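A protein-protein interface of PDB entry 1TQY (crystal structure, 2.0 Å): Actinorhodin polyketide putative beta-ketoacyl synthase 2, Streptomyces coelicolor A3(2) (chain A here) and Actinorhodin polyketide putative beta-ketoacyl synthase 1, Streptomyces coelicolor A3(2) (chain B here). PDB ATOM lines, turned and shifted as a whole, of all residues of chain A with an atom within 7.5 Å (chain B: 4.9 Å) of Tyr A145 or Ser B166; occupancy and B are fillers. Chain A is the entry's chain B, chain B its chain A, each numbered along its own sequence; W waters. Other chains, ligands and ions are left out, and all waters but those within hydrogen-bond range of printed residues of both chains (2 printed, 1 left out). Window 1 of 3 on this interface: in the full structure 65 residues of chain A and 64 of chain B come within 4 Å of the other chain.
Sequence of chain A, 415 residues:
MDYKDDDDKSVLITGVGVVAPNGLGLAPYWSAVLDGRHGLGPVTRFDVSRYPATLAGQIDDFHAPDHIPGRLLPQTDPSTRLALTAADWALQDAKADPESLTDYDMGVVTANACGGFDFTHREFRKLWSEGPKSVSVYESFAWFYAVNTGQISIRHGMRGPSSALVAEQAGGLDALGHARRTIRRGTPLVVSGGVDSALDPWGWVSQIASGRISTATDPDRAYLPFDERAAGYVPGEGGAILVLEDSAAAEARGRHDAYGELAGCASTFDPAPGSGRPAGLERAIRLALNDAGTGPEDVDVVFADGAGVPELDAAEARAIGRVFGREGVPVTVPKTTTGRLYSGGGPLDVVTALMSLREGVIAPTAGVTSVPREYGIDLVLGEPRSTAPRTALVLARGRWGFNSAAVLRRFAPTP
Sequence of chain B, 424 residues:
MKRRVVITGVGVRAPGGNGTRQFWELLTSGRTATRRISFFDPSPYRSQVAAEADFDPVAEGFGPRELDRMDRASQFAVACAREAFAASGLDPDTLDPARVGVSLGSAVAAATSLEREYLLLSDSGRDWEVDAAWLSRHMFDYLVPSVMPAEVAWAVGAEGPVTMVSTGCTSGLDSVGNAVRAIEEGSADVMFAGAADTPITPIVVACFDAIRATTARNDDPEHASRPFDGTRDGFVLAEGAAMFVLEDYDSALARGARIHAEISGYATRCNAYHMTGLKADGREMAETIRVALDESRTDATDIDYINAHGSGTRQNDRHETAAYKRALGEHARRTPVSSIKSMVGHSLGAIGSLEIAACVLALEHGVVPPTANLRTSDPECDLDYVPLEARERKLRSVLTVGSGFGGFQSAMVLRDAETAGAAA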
ATOM      1  N   THR A 110       3.967  27.316  -6.993  1.00  0.00           N
ATOM      2  CA  THR A 110       5.024  27.820  -7.862  1.00  0.00           C
ATOM      3  C   THR A 110       4.504  28.281  -9.196  1.00  0.00           C
ATOM      4  O   THR A 110       3.390  27.946  -9.584  1.00  0.00           O
ATOM      5  CB  THR A 110       6.063  26.733  -8.204  1.00  0.00           C
ATOM      6  OG1 THR A 110       5.404  25.666  -8.904  1.00  0.00           O
ATOM      7  CG2 THR A 110       6.748  26.212  -6.946  1.00  0.00           C
ATOM      8  N   ALA A 111       5.317  29.060  -9.898  1.00  0.00           N
ATOM      9  CA  ALA A 111       4.952  29.485 -11.243  1.00  0.00           C
ATOM     10  C   ALA A 111       6.008  28.822 -12.136  1.00  0.00           C
ATOM     11  O   ALA A 111       7.138  28.606 -11.703  1.00  0.00           O
ATOM     12  CB  ALA A 111       5.019  31.003 -11.367  1.00  0.00           C
ATOM     13  N   ASN A 112       5.642  28.472 -13.361  1.00  0.00           N
ATOM     14  CA  ASN A 112       6.590  27.847 -14.281  1.00  0.00           C
ATOM     15  C   ASN A 112       6.263  28.349 -15.683  1.00  0.00           C
ATOM     16  O   ASN A 112       5.121  28.269 -16.124  1.00  0.00           O
ATOM     17  CB  ASN A 112       6.456  26.321 -14.233  1.00  0.00           C
ATOM     18  CG  ASN A 112       7.730  25.616 -14.633  1.00  0.00           C
ATOM     19  OD1 ASN A 112       8.422  26.044 -15.565  1.00  0.00           O
ATOM     20  ND2 ASN A 112       8.049  24.522 -13.938  1.00  0.00           N
ATOM     21  N   ALA A 113       7.251  28.870 -16.392  1.00  0.00           N
ATOM     22  CA  ALA A 113       6.987  29.393 -17.726  1.00  0.00           C
ATOM     23  C   ALA A 113       7.354  28.463 -18.886  1.00  0.00           C
ATOM     24  O   ALA A 113       6.572  28.289 -19.823  1.00  0.00           O
ATOM     25  CB  ALA A 113       7.703  30.727 -17.888  1.00  0.00           C
ATOM     26  N   CYS A 114       8.544  27.869 -18.816  1.00  0.00           N
ATOM     27  CA  CYS A 114       9.056  26.990 -19.867  1.00  0.00           C
ATOM     28  C   CYS A 114       8.991  25.520 -19.512  1.00  0.00           C
ATOM     29  O   CYS A 114       9.037  24.672 -20.395  1.00  0.00           O
ATOM     30  CB  CYS A 114      10.517  27.324 -20.159  1.00  0.00           C
ATOM     31  SG  CYS A 114      10.834  29.076 -20.382  1.00  0.00           S
ATOM     32  N   GLY A 115       8.903  25.225 -18.219  1.00  0.00           N
ATOM     33  CA  GLY A 115       8.880  23.840 -17.786  1.00  0.00           C
ATOM     34  C   GLY A 115      10.269  23.264 -18.006  1.00  0.00           C
ATOM     35  O   GLY A 115      11.224  24.014 -18.228  1.00  0.00           O
ATOM     36  N   GLY A 116      10.389  21.940 -17.961  1.00  0.00           N
ATOM     37  CA  GLY A 116      11.683  21.315 -18.165  1.00  0.00           C
ATOM     38  C   GLY A 116      11.997  21.212 -19.638  1.00  0.00           C
ATOM     39  O   GLY A 116      12.040  20.118 -20.182  1.00  0.00           O
ATOM     40  N   PHE A 117      12.239  22.351 -20.286  1.00  0.00           N
ATOM     41  CA  PHE A 117      12.496  22.356 -21.716  1.00  0.00           C
ATOM     42  C   PHE A 117      13.784  21.660 -22.188  1.00  0.00           C
ATOM     43  O   PHE A 117      13.748  20.971 -23.199  1.00  0.00           O
ATOM     44  CB  PHE A 117      12.436  23.785 -22.261  1.00  0.00           C
ATOM     45  CG  PHE A 117      11.935  23.858 -23.678  1.00  0.00           C
ATOM     46  CD1 PHE A 117      10.607  23.573 -23.970  1.00  0.00           C
ATOM     47  CD2 PHE A 117      12.804  24.132 -24.726  1.00  0.00           C
ATOM     48  CE1 PHE A 117      10.148  23.555 -25.282  1.00  0.00           C
ATOM     49  CE2 PHE A 117      12.351  24.115 -26.046  1.00  0.00           C
ATOM     50  CZ  PHE A 117      11.021  23.823 -26.321  1.00  0.00           C
ATOM     51  N   PHE A 141       6.998  13.311 -16.472  1.00  0.00           N
ATOM     52  CA  PHE A 141       6.820  14.308 -15.423  1.00  0.00           C
ATOM     53  C   PHE A 141       7.969  15.298 -15.248  1.00  0.00           C
ATOM     54  O   PHE A 141       7.887  16.192 -14.409  1.00  0.00           O
ATOM     55  CB  PHE A 141       6.554  13.624 -14.082  1.00  0.00           C
ATOM     56  CG  PHE A 141       7.717  12.818 -13.572  1.00  0.00           C
ATOM     57  CD1 PHE A 141       7.756  11.439 -13.742  1.00  0.00           C
ATOM     58  CD2 PHE A 141       8.773  13.441 -12.919  1.00  0.00           C
ATOM     59  CE1 PHE A 141       8.832  10.689 -13.272  1.00  0.00           C
ATOM     60  CE2 PHE A 141       9.855  12.699 -12.445  1.00  0.00           C
ATOM     61  CZ  PHE A 141       9.879  11.321 -12.621  1.00  0.00           C
ATOM     62  N   ALA A 142       9.040  15.141 -16.021  1.00  0.00           N
ATOM     63  CA  ALA A 142      10.187  16.046 -15.913  1.00  0.00           C
ATOM     64  C   ALA A 142       9.966  17.354 -16.658  1.00  0.00           C
ATOM     65  O   ALA A 142      10.618  18.350 -16.364  1.00  0.00           O
ATOM     66  CB  ALA A 142      11.433  15.366 -16.439  1.00  0.00           C
ATOM     67  N   TRP A 143       9.040  17.351 -17.609  1.00  0.00           N
ATOM     68  CA  TRP A 143       8.761  18.538 -18.412  1.00  0.00           C
ATOM     69  C   TRP A 143       7.545  19.381 -18.011  1.00  0.00           C
ATOM     70  O   TRP A 143       7.651  20.601 -17.940  1.00  0.00           O
ATOM     71  CB  TRP A 143       8.588  18.126 -19.874  1.00  0.00           C
ATOM     72  CG  TRP A 143       7.995  19.213 -20.739  1.00  0.00           C
ATOM     73  CD1 TRP A 143       8.558  20.423 -21.033  1.00  0.00           C
ATOM     74  CD2 TRP A 143       6.707  19.206 -21.371  1.00  0.00           C
ATOM     75  NE1 TRP A 143       7.698  21.169 -21.805  1.00  0.00           N
ATOM     76  CE2 TRP A 143       6.556  20.446 -22.026  1.00  0.00           C
ATOM     77  CE3 TRP A 143       5.664  18.272 -21.444  1.00  0.00           C
ATOM     78  CZ2 TRP A 143       5.404  20.783 -22.746  1.00  0.00           C
ATOM     79  CZ3 TRP A 143       4.517  18.604 -22.161  1.00  0.00           C
ATOM     80  CH2 TRP A 143       4.399  19.854 -22.802  1.00  0.00           C
ATOM     81  N   PHE A 144       6.402  18.732 -17.768  1.00  0.00           N
ATOM     82  CA  PHE A 144       5.165  19.444 -17.457  1.00  0.00           C
ATOM     83  C   PHE A 144       5.335  20.595 -16.462  1.00  0.00           C
ATOM     84  O   PHE A 144       6.228  20.579 -15.602  1.00  0.00           O
ATOM     85  CB  PHE A 144       4.018  18.453 -17.080  1.00  0.00           C
ATOM     86  CG  PHE A 144       4.007  17.973 -15.638  1.00  0.00           C
ATOM     87  CD1 PHE A 144       5.183  17.647 -14.967  1.00  0.00           C
ATOM     88  CD2 PHE A 144       2.784  17.788 -14.976  1.00  0.00           C
ATOM     89  CE1 PHE A 144       5.146  17.138 -13.644  1.00  0.00           C
ATOM     90  CE2 PHE A 144       2.729  17.283 -13.664  1.00  0.00           C
ATOM     91  CZ  PHE A 144       3.912  16.957 -12.995  1.00  0.00           C
ATOM     92  N   TYR A 145       4.498  21.617 -16.620  1.00  0.00           N
ATOM     93  CA  TYR A 145       4.592  22.826 -15.810  1.00  0.00           C
ATOM     94  C   TYR A 145       4.476  22.657 -14.305  1.00  0.00           C
ATOM     95  O   TYR A 145       5.063  23.421 -13.554  1.00  0.00           O
ATOM     96  CB  TYR A 145       3.589  23.846 -16.348  1.00  0.00           C
ATOM     97  CG  TYR A 145       3.823  24.058 -17.831  1.00  0.00           C
ATOM     98  CD1 TYR A 145       4.916  24.802 -18.289  1.00  0.00           C
ATOM     99  CD2 TYR A 145       3.061  23.368 -18.776  1.00  0.00           C
ATOM    100  CE1 TYR A 145       5.251  24.837 -19.647  1.00  0.00           C
ATOM    101  CE2 TYR A 145       3.390  23.393 -20.135  1.00  0.00           C
ATOM    102  CZ  TYR A 145       4.494  24.126 -20.558  1.00  0.00           C
ATOM    103  OH  TYR A 145       4.860  24.087 -21.883  1.00  0.00           O
ATOM    104  N   ALA A 146       3.746  21.639 -13.861  1.00  0.00           N
ATOM    105  CA  ALA A 146       3.593  21.399 -12.433  1.00  0.00           C
ATOM    106  C   ALA A 146       4.824  20.765 -11.780  1.00  0.00           C
ATOM    107  O   ALA A 146       4.917  20.738 -10.557  1.00  0.00           O
ATOM    108  CB  ALA A 146       2.388  20.503 -12.190  1.00  0.00           C
ATOM    109  N   VAL A 147       5.771  20.288 -12.583  1.00  0.00           N
ATOM    110  CA  VAL A 147       6.938  19.585 -12.048  1.00  0.00           C
ATOM    111  C   VAL A 147       7.573  20.116 -10.766  1.00  0.00           C
ATOM    112  O   VAL A 147       7.729  19.362  -9.805  1.00  0.00           O
ATOM    113  CB  VAL A 147       8.060  19.384 -13.138  1.00  0.00           C
ATOM    114  CG1 VAL A 147       8.641  20.731 -13.599  1.00  0.00           C
ATOM    115  CG2 VAL A 147       9.158  18.490 -12.576  1.00  0.00           C
ATOM    116  N   ASN A 148       7.908  21.399 -10.715  1.00  0.00           N
ATOM    117  CA  ASN A 148       8.544  21.922  -9.513  1.00  0.00           C
ATOM    118  C   ASN A 148       7.684  21.940  -8.255  1.00  0.00           C
ATOM    119  O   ASN A 148       8.204  21.895  -7.137  1.00  0.00           O
ATOM    120  CB  ASN A 148       9.129  23.296  -9.793  1.00  0.00           C
ATOM    121  CG  ASN A 148      10.077  23.262 -10.956  1.00  0.00           C
ATOM    122  OD1 ASN A 148      10.815  22.282 -11.126  1.00  0.00           O
ATOM    123  ND2 ASN A 148      10.068  24.305 -11.774  1.00  0.00           N
ATOM    124  N   THR A 149       6.370  21.996  -8.416  1.00  0.00           N
ATOM    125  CA  THR A 149       5.518  21.977  -7.235  1.00  0.00           C
ATOM    126  C   THR A 149       5.503  20.543  -6.694  1.00  0.00           C
ATOM    127  O   THR A 149       5.729  20.313  -5.504  1.00  0.00           O
ATOM    128  CB  THR A 149       4.084  22.446  -7.559  1.00  0.00           C
ATOM    129  OG1 THR A 149       4.089  23.863  -7.783  1.00  0.00           O
ATOM    130  CG2 THR A 149       3.146  22.139  -6.409  1.00  0.00           C
ATOM    131  N   GLY A 150       5.272  19.587  -7.585  1.00  0.00           N
ATOM    132  CA  GLY A 150       5.249  18.193  -7.187  1.00  0.00           C
ATOM    133  C   GLY A 150       6.553  17.677  -6.597  1.00  0.00           C
ATOM    134  O   GLY A 150       6.531  16.884  -5.656  1.00  0.00           O
ATOM    135  N   SER A 163      -0.297  24.294  -5.891  1.00  0.00           N
ATOM    136  CA  SER A 163      -0.614  24.596  -7.289  1.00  0.00           C
ATOM    137  C   SER A 163       0.594  25.037  -8.100  1.00  0.00           C
ATOM    138  O   SER A 163       1.690  25.229  -7.572  1.00  0.00           O
ATOM    139  CB  SER A 163      -1.697  25.683  -7.363  1.00  0.00           C
ATOM    140  OG  SER A 163      -2.354  25.662  -8.626  1.00  0.00           O
ATOM    141  N   ALA A 164       0.374  25.159  -9.402  1.00  0.00           N
ATOM    142  CA  ALA A 164       1.392  25.607 -10.350  1.00  0.00           C
ATOM    143  C   ALA A 164       0.631  26.488 -11.329  1.00  0.00           C
ATOM    144  O   ALA A 164      -0.434  26.112 -11.821  1.00  0.00           O
ATOM    145  CB  ALA A 164       2.026  24.423 -11.080  1.00  0.00           C
ATOM    146  N   LEU A 165       1.194  27.656 -11.601  1.00  0.00           N
ATOM    147  CA  LEU A 165       0.578  28.637 -12.473  1.00  0.00           C
ATOM    148  C   LEU A 165       1.522  28.973 -13.610  1.00  0.00           C
ATOM    149  O   LEU A 165       2.730  28.808 -13.480  1.00  0.00           O
ATOM    150  CB  LEU A 165       0.296  29.916 -11.674  1.00  0.00           C
ATOM    151  CG  LEU A 165      -0.530  29.788 -10.396  1.00  0.00           C
ATOM    152  CD1 LEU A 165      -0.705  31.155  -9.739  1.00  0.00           C
ATOM    153  CD2 LEU A 165      -1.881  29.194 -10.731  1.00  0.00           C
ATOM    154  N   VAL A 166       0.963  29.415 -14.732  1.00  0.00           N
ATOM    155  CA  VAL A 166       1.762  29.829 -15.875  1.00  0.00           C
ATOM    156  C   VAL A 166       1.202  31.163 -16.377  1.00  0.00           C
ATOM    157  O   VAL A 166       0.026  31.256 -16.726  1.00  0.00           O
ATOM    158  CB  VAL A 166       1.718  28.800 -17.047  1.00  0.00           C
ATOM    159  CG1 VAL A 166       2.597  29.307 -18.193  1.00  0.00           C
ATOM    160  CG2 VAL A 166       2.217  27.426 -16.585  1.00  0.00           C
ATOM    161  N   ASP A 196      13.098  29.339 -13.734  1.00  0.00           N
ATOM    162  CA  ASP A 196      12.995  28.935 -15.133  1.00  0.00           C
ATOM    163  C   ASP A 196      14.403  28.810 -15.667  1.00  0.00           C
ATOM    164  O   ASP A 196      15.342  29.343 -15.080  1.00  0.00           O
ATOM    165  CB  ASP A 196      12.238  29.964 -15.996  1.00  0.00           C
ATOM    166  CG  ASP A 196      10.763  29.635 -16.163  1.00  0.00           C
ATOM    167  OD1 ASP A 196       9.924  30.300 -15.502  1.00  0.00           O
ATOM    168  OD2 ASP A 196      10.428  28.720 -16.960  1.00  0.00           O
ATOM    169  N   SER B 106      -4.541  23.354 -18.096  1.00  0.00           N
ATOM    170  CA  SER B 106      -3.958  22.571 -19.167  1.00  0.00           C
ATOM    171  C   SER B 106      -2.744  21.831 -18.648  1.00  0.00           C
ATOM    172  O   SER B 106      -1.859  22.425 -18.015  1.00  0.00           O
ATOM    173  CB  SER B 106      -3.561  23.481 -20.328  1.00  0.00           C
ATOM    174  OG  SER B 106      -3.115  22.706 -21.429  1.00  0.00           O
ATOM    175  N   ALA B 107      -2.708  20.532 -18.920  1.00  0.00           N
ATOM    176  CA  ALA B 107      -1.613  19.671 -18.491  1.00  0.00           C
ATOM    177  C   ALA B 107      -0.392  19.758 -19.412  1.00  0.00           C
ATOM    178  O   ALA B 107       0.699  20.076 -18.943  1.00  0.00           O
ATOM    179  CB  ALA B 107      -2.103  18.229 -18.406  1.00  0.00           C
ATOM    180  N   VAL B 108      -0.582  19.490 -20.709  1.00  0.00           N
ATOM    181  CA  VAL B 108       0.517  19.522 -21.680  1.00  0.00           C
ATOM    182  C   VAL B 108       0.483  20.688 -22.675  1.00  0.00           C
ATOM    183  O   VAL B 108       1.343  20.777 -23.549  1.00  0.00           O
ATOM    184  CB  VAL B 108       0.592  18.237 -22.529  1.00  0.00           C
ATOM    185  CG1 VAL B 108       0.769  17.029 -21.627  1.00  0.00           C
ATOM    186  CG2 VAL B 108      -0.634  18.122 -23.414  1.00  0.00           C
ATOM    187  N   ALA B 109      -0.527  21.544 -22.565  1.00  0.00           N
ATOM    188  CA  ALA B 109      -0.656  22.731 -23.403  1.00  0.00           C
ATOM    189  C   ALA B 109      -0.374  22.633 -24.909  1.00  0.00           C
ATOM    190  O   ALA B 109      -1.136  22.022 -25.659  1.00  0.00           O
ATOM    191  CB  ALA B 109       0.205  23.841 -22.805  1.00  0.00           C
ATOM    192  N   TYR B 142       4.593  28.674 -27.823  1.00  0.00           N
ATOM    193  CA  TYR B 142       4.386  27.248 -27.649  1.00  0.00           C
ATOM    194  C   TYR B 142       5.323  26.889 -26.507  1.00  0.00           C
ATOM    195  O   TYR B 142       5.044  25.991 -25.710  1.00  0.00           O
ATOM    196  CB  TYR B 142       4.744  26.486 -28.921  1.00  0.00           C
ATOM    197  CG  TYR B 142       3.940  26.960 -30.102  1.00  0.00           C
ATOM    198  CD1 TYR B 142       4.482  26.955 -31.377  1.00  0.00           C
ATOM    199  CD2 TYR B 142       2.655  27.479 -29.930  1.00  0.00           C
ATOM    200  CE1 TYR B 142       3.771  27.466 -32.460  1.00  0.00           C
ATOM    201  CE2 TYR B 142       1.938  27.988 -31.001  1.00  0.00           C
ATOM    202  CZ  TYR B 142       2.508  27.979 -32.266  1.00  0.00           C
ATOM    203  OH  TYR B 142       1.823  28.494 -33.339  1.00  0.00           O
ATOM    204  N   LEU B 143       6.438  27.607 -26.419  1.00  0.00           N
ATOM    205  CA  LEU B 143       7.400  27.384 -25.337  1.00  0.00           C
ATOM    206  C   LEU B 143       6.773  27.774 -23.990  1.00  0.00           C
ATOM    207  O   LEU B 143       6.915  27.064 -22.996  1.00  0.00           O
ATOM    208  CB  LEU B 143       8.671  28.222 -25.569  1.00  0.00           C
ATOM    209  CG  LEU B 143       9.642  28.302 -24.371  1.00  0.00           C
ATOM    210  CD1 LEU B 143      10.274  26.938 -24.127  1.00  0.00           C
ATOM    211  CD2 LEU B 143      10.719  29.334 -24.629  1.00  0.00           C
ATOM    212  N   PRO B 145       3.138  28.515 -22.727  1.00  0.00           N
ATOM    213  CA  PRO B 145       1.692  28.340 -22.961  1.00  0.00           C
ATOM    214  C   PRO B 145       0.737  29.443 -22.487  1.00  0.00           C
ATOM    215  O   PRO B 145      -0.469  29.364 -22.744  1.00  0.00           O
ATOM    216  CB  PRO B 145       1.370  27.025 -22.248  1.00  0.00           C
ATOM    217  CG  PRO B 145       2.687  26.353 -22.078  1.00  0.00           C
ATOM    218  CD  PRO B 145       3.628  27.478 -21.802  1.00  0.00           C
ATOM    219  N   MET B 164      -3.211  30.736 -16.126  1.00  0.00           N
ATOM    220  CA  MET B 164      -3.225  29.336 -16.511  1.00  0.00           C
ATOM    221  C   MET B 164      -2.892  28.539 -15.261  1.00  0.00           C
ATOM    222  O   MET B 164      -1.987  28.894 -14.521  1.00  0.00           O
ATOM    223  CB  MET B 164      -2.174  29.055 -17.590  1.00  0.00           C
ATOM    224  CG  MET B 164      -2.100  27.594 -18.011  1.00  0.00           C
ATOM    225  SD  MET B 164      -1.227  27.340 -19.586  1.00  0.00           S
ATOM    226  CE  MET B 164      -0.115  26.061 -19.122  1.00  0.00           C
ATOM    227  N   VAL B 165      -3.658  27.488 -15.012  1.00  0.00           N
ATOM    228  CA  VAL B 165      -3.408  26.614 -13.874  1.00  0.00           C
ATOM    229  C   VAL B 165      -2.945  25.341 -14.582  1.00  0.00           C
ATOM    230  O   VAL B 165      -3.606  24.862 -15.509  1.00  0.00           O
ATOM    231  CB  VAL B 165      -4.696  26.385 -13.038  1.00  0.00           C
ATOM    232  CG1 VAL B 165      -4.409  25.486 -11.838  1.00  0.00           C
ATOM    233  CG2 VAL B 165      -5.241  27.730 -12.542  1.00  0.00           C
ATOM    234  N   SER B 166      -1.793  24.820 -14.177  1.00  0.00           N
ATOM    235  CA  SER B 166      -1.226  23.631 -14.810  1.00  0.00           C
ATOM    236  C   SER B 166      -0.793  22.659 -13.723  1.00  0.00           C
ATOM    237  O   SER B 166       0.364  22.657 -13.321  1.00  0.00           O
ATOM    238  CB  SER B 166      -0.024  24.045 -15.674  1.00  0.00           C
ATOM    239  OG  SER B 166       0.431  22.994 -16.522  1.00  0.00           O
ATOM    240  N   THR B 167      -1.731  21.844 -13.240  1.00  0.00           N
ATOM    241  CA  THR B 167      -1.437  20.875 -12.186  1.00  0.00           C
ATOM    242  C   THR B 167      -1.644  19.454 -12.682  1.00  0.00           C
ATOM    243  O   THR B 167      -2.295  18.639 -12.023  1.00  0.00           O
ATOM    244  CB  THR B 167      -2.337  21.086 -10.960  1.00  0.00           C
ATOM    245  OG1 THR B 167      -3.701  21.194 -11.387  1.00  0.00           O
ATOM    246  CG2 THR B 167      -1.928  22.340 -10.200  1.00  0.00           C
ATOM    247  N   GLY B 168      -1.102  19.167 -13.860  1.00  0.00           N
ATOM    248  CA  GLY B 168      -1.225  17.840 -14.421  1.00  0.00           C
ATOM    249  C   GLY B 168      -2.644  17.418 -14.732  1.00  0.00           C
ATOM    250  O   GLY B 168      -3.424  18.168 -15.326  1.00  0.00           O
ATOM    251  N   SER B 171      -5.726  19.642 -13.478  1.00  0.00           N
ATOM    252  CA  SER B 171      -5.893  21.009 -14.004  1.00  0.00           C
ATOM    253  C   SER B 171      -7.368  21.376 -14.246  1.00  0.00           C
ATOM    254  O   SER B 171      -7.808  22.469 -13.894  1.00  0.00           O
ATOM    255  CB  SER B 171      -5.131  21.196 -15.336  1.00  0.00           C
ATOM    256  OG  SER B 171      -3.743  21.019 -15.206  1.00  0.00           O
HETATM  257  O   HOH W   1       3.351  24.319 -24.482  1.00  0.00           O
HETATM  258  O   HOH W   2       7.372  24.504 -22.352  1.00  0.00           O
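The backbone carbonyl oxygen (O) of Met B164 lies within hydrogen-bond range of the backbone NH (N) of Val A166, 3.0 Å away.
N of Ser B166 lies within hydrogen-bond range of O of Ala A164, 3.0 Å away.
O of Ala A113 lies close to O of Leu B143 (3.4 Å).
N of Ser B106 is in hydrogen-bond range of O of Val B165.
The backbone carbonyl oxygen (O) of Ser A163 is in hydrogen-bond range of the backbone NH (N) of Thr A110, at 3.1 Å.
The side-chain amide nitrogen (ND2) of Asn A112 sits at hydrogen-bond distance from the backbone carbonyl oxygen (O) of Tyr A145 (3.2 Å).
The backbone carbonyl oxygen (O) of Leu A165 sits at hydrogen-bond distance from the backbone NH (N) of Asn A112 (2.9 Å).
The backbone NH (N) of Ala A113 sits at hydrogen-bond distance from the side-chain carboxylate (OD1) of Asp A196 (3.2 Å).
The backbone carbonyl oxygen (O) of Trp A143 sits at hydrogen-bond distance from the backbone NH (N) of Gly A116 (3.0 Å).
Among the printed residues, merely in contact across the chains: Tyr A145 with Pro B145 (3.1 Å), Ala A146 with Ser B166 (3.2 Å), Tyr A145 with Ser B166 (3.3 Å), Trp A143 with Val B108 (3.3 Å), Leu A165 with Met B164 (3.3 Å), Phe A117 with Leu B143 (3.4 Å), Ala A113 with Pro B145 (3.6 Å), Ala A164 with Val B165 (3.6 Å), Ser A163 with Thr B167 (3.7 Å), Ala A164 with Thr B167 (3.7 Å), Tyr A145 with Leu B143 (3.8 Å), Cys A114 with Leu B143 (3.8 Å), Ser A163 with Val B165 (3.8 Å) and Ala A146 with Thr B167 (3.8 Å).
Of the printed residues of chain B, Cys A114 touches Leu B143 (3.8 Å).
Printed residues of chain B within 4 Å of Trp A143: Val B108.
Tyr A145 touches just these residues of chain B: Leu B143, Pro B145 and Ser B166.
Asp A196 touches none of the printed residues of chain B.
Of the printed residues of chain A, Met B164 touches Leu A165 and Val A166.
Ser B166 touches just these residues of chain A: Tyr A145 (3.3 Å), Ala A146 (3.2 Å) and Ala A164 (3.0 Å).
The nearest printed residue of chain B that does not touch Leu A165 is Val B165 (4.1 Å).
Hydrophobic or aromatic side chains of chain B within 4 Å of the printed part of chain A: Val B108, Leu B143, Pro B145, Met B164 and Val B165.
Hydrophobic or aromatic side chains of chain A that line the printed part of chain B: Phe A117, Trp A143, Tyr A145, Ala A146, Ala A164, Leu A165 and Val A166.
Among the printed residues, 17 pairs touch across the chains.
Water W2 lies within hydrogen-bond range of O of Cys A114 (2.6 Å), OH of Tyr A145 (2.6 Å), O of Leu B143 (2.7 Å) and NE1 of Trp A143 (3.4 Å).
Water W1 lies within hydrogen-bond range of O of Tyr B142 (2.7 Å) and OH of Tyr A145 (3.0 Å).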
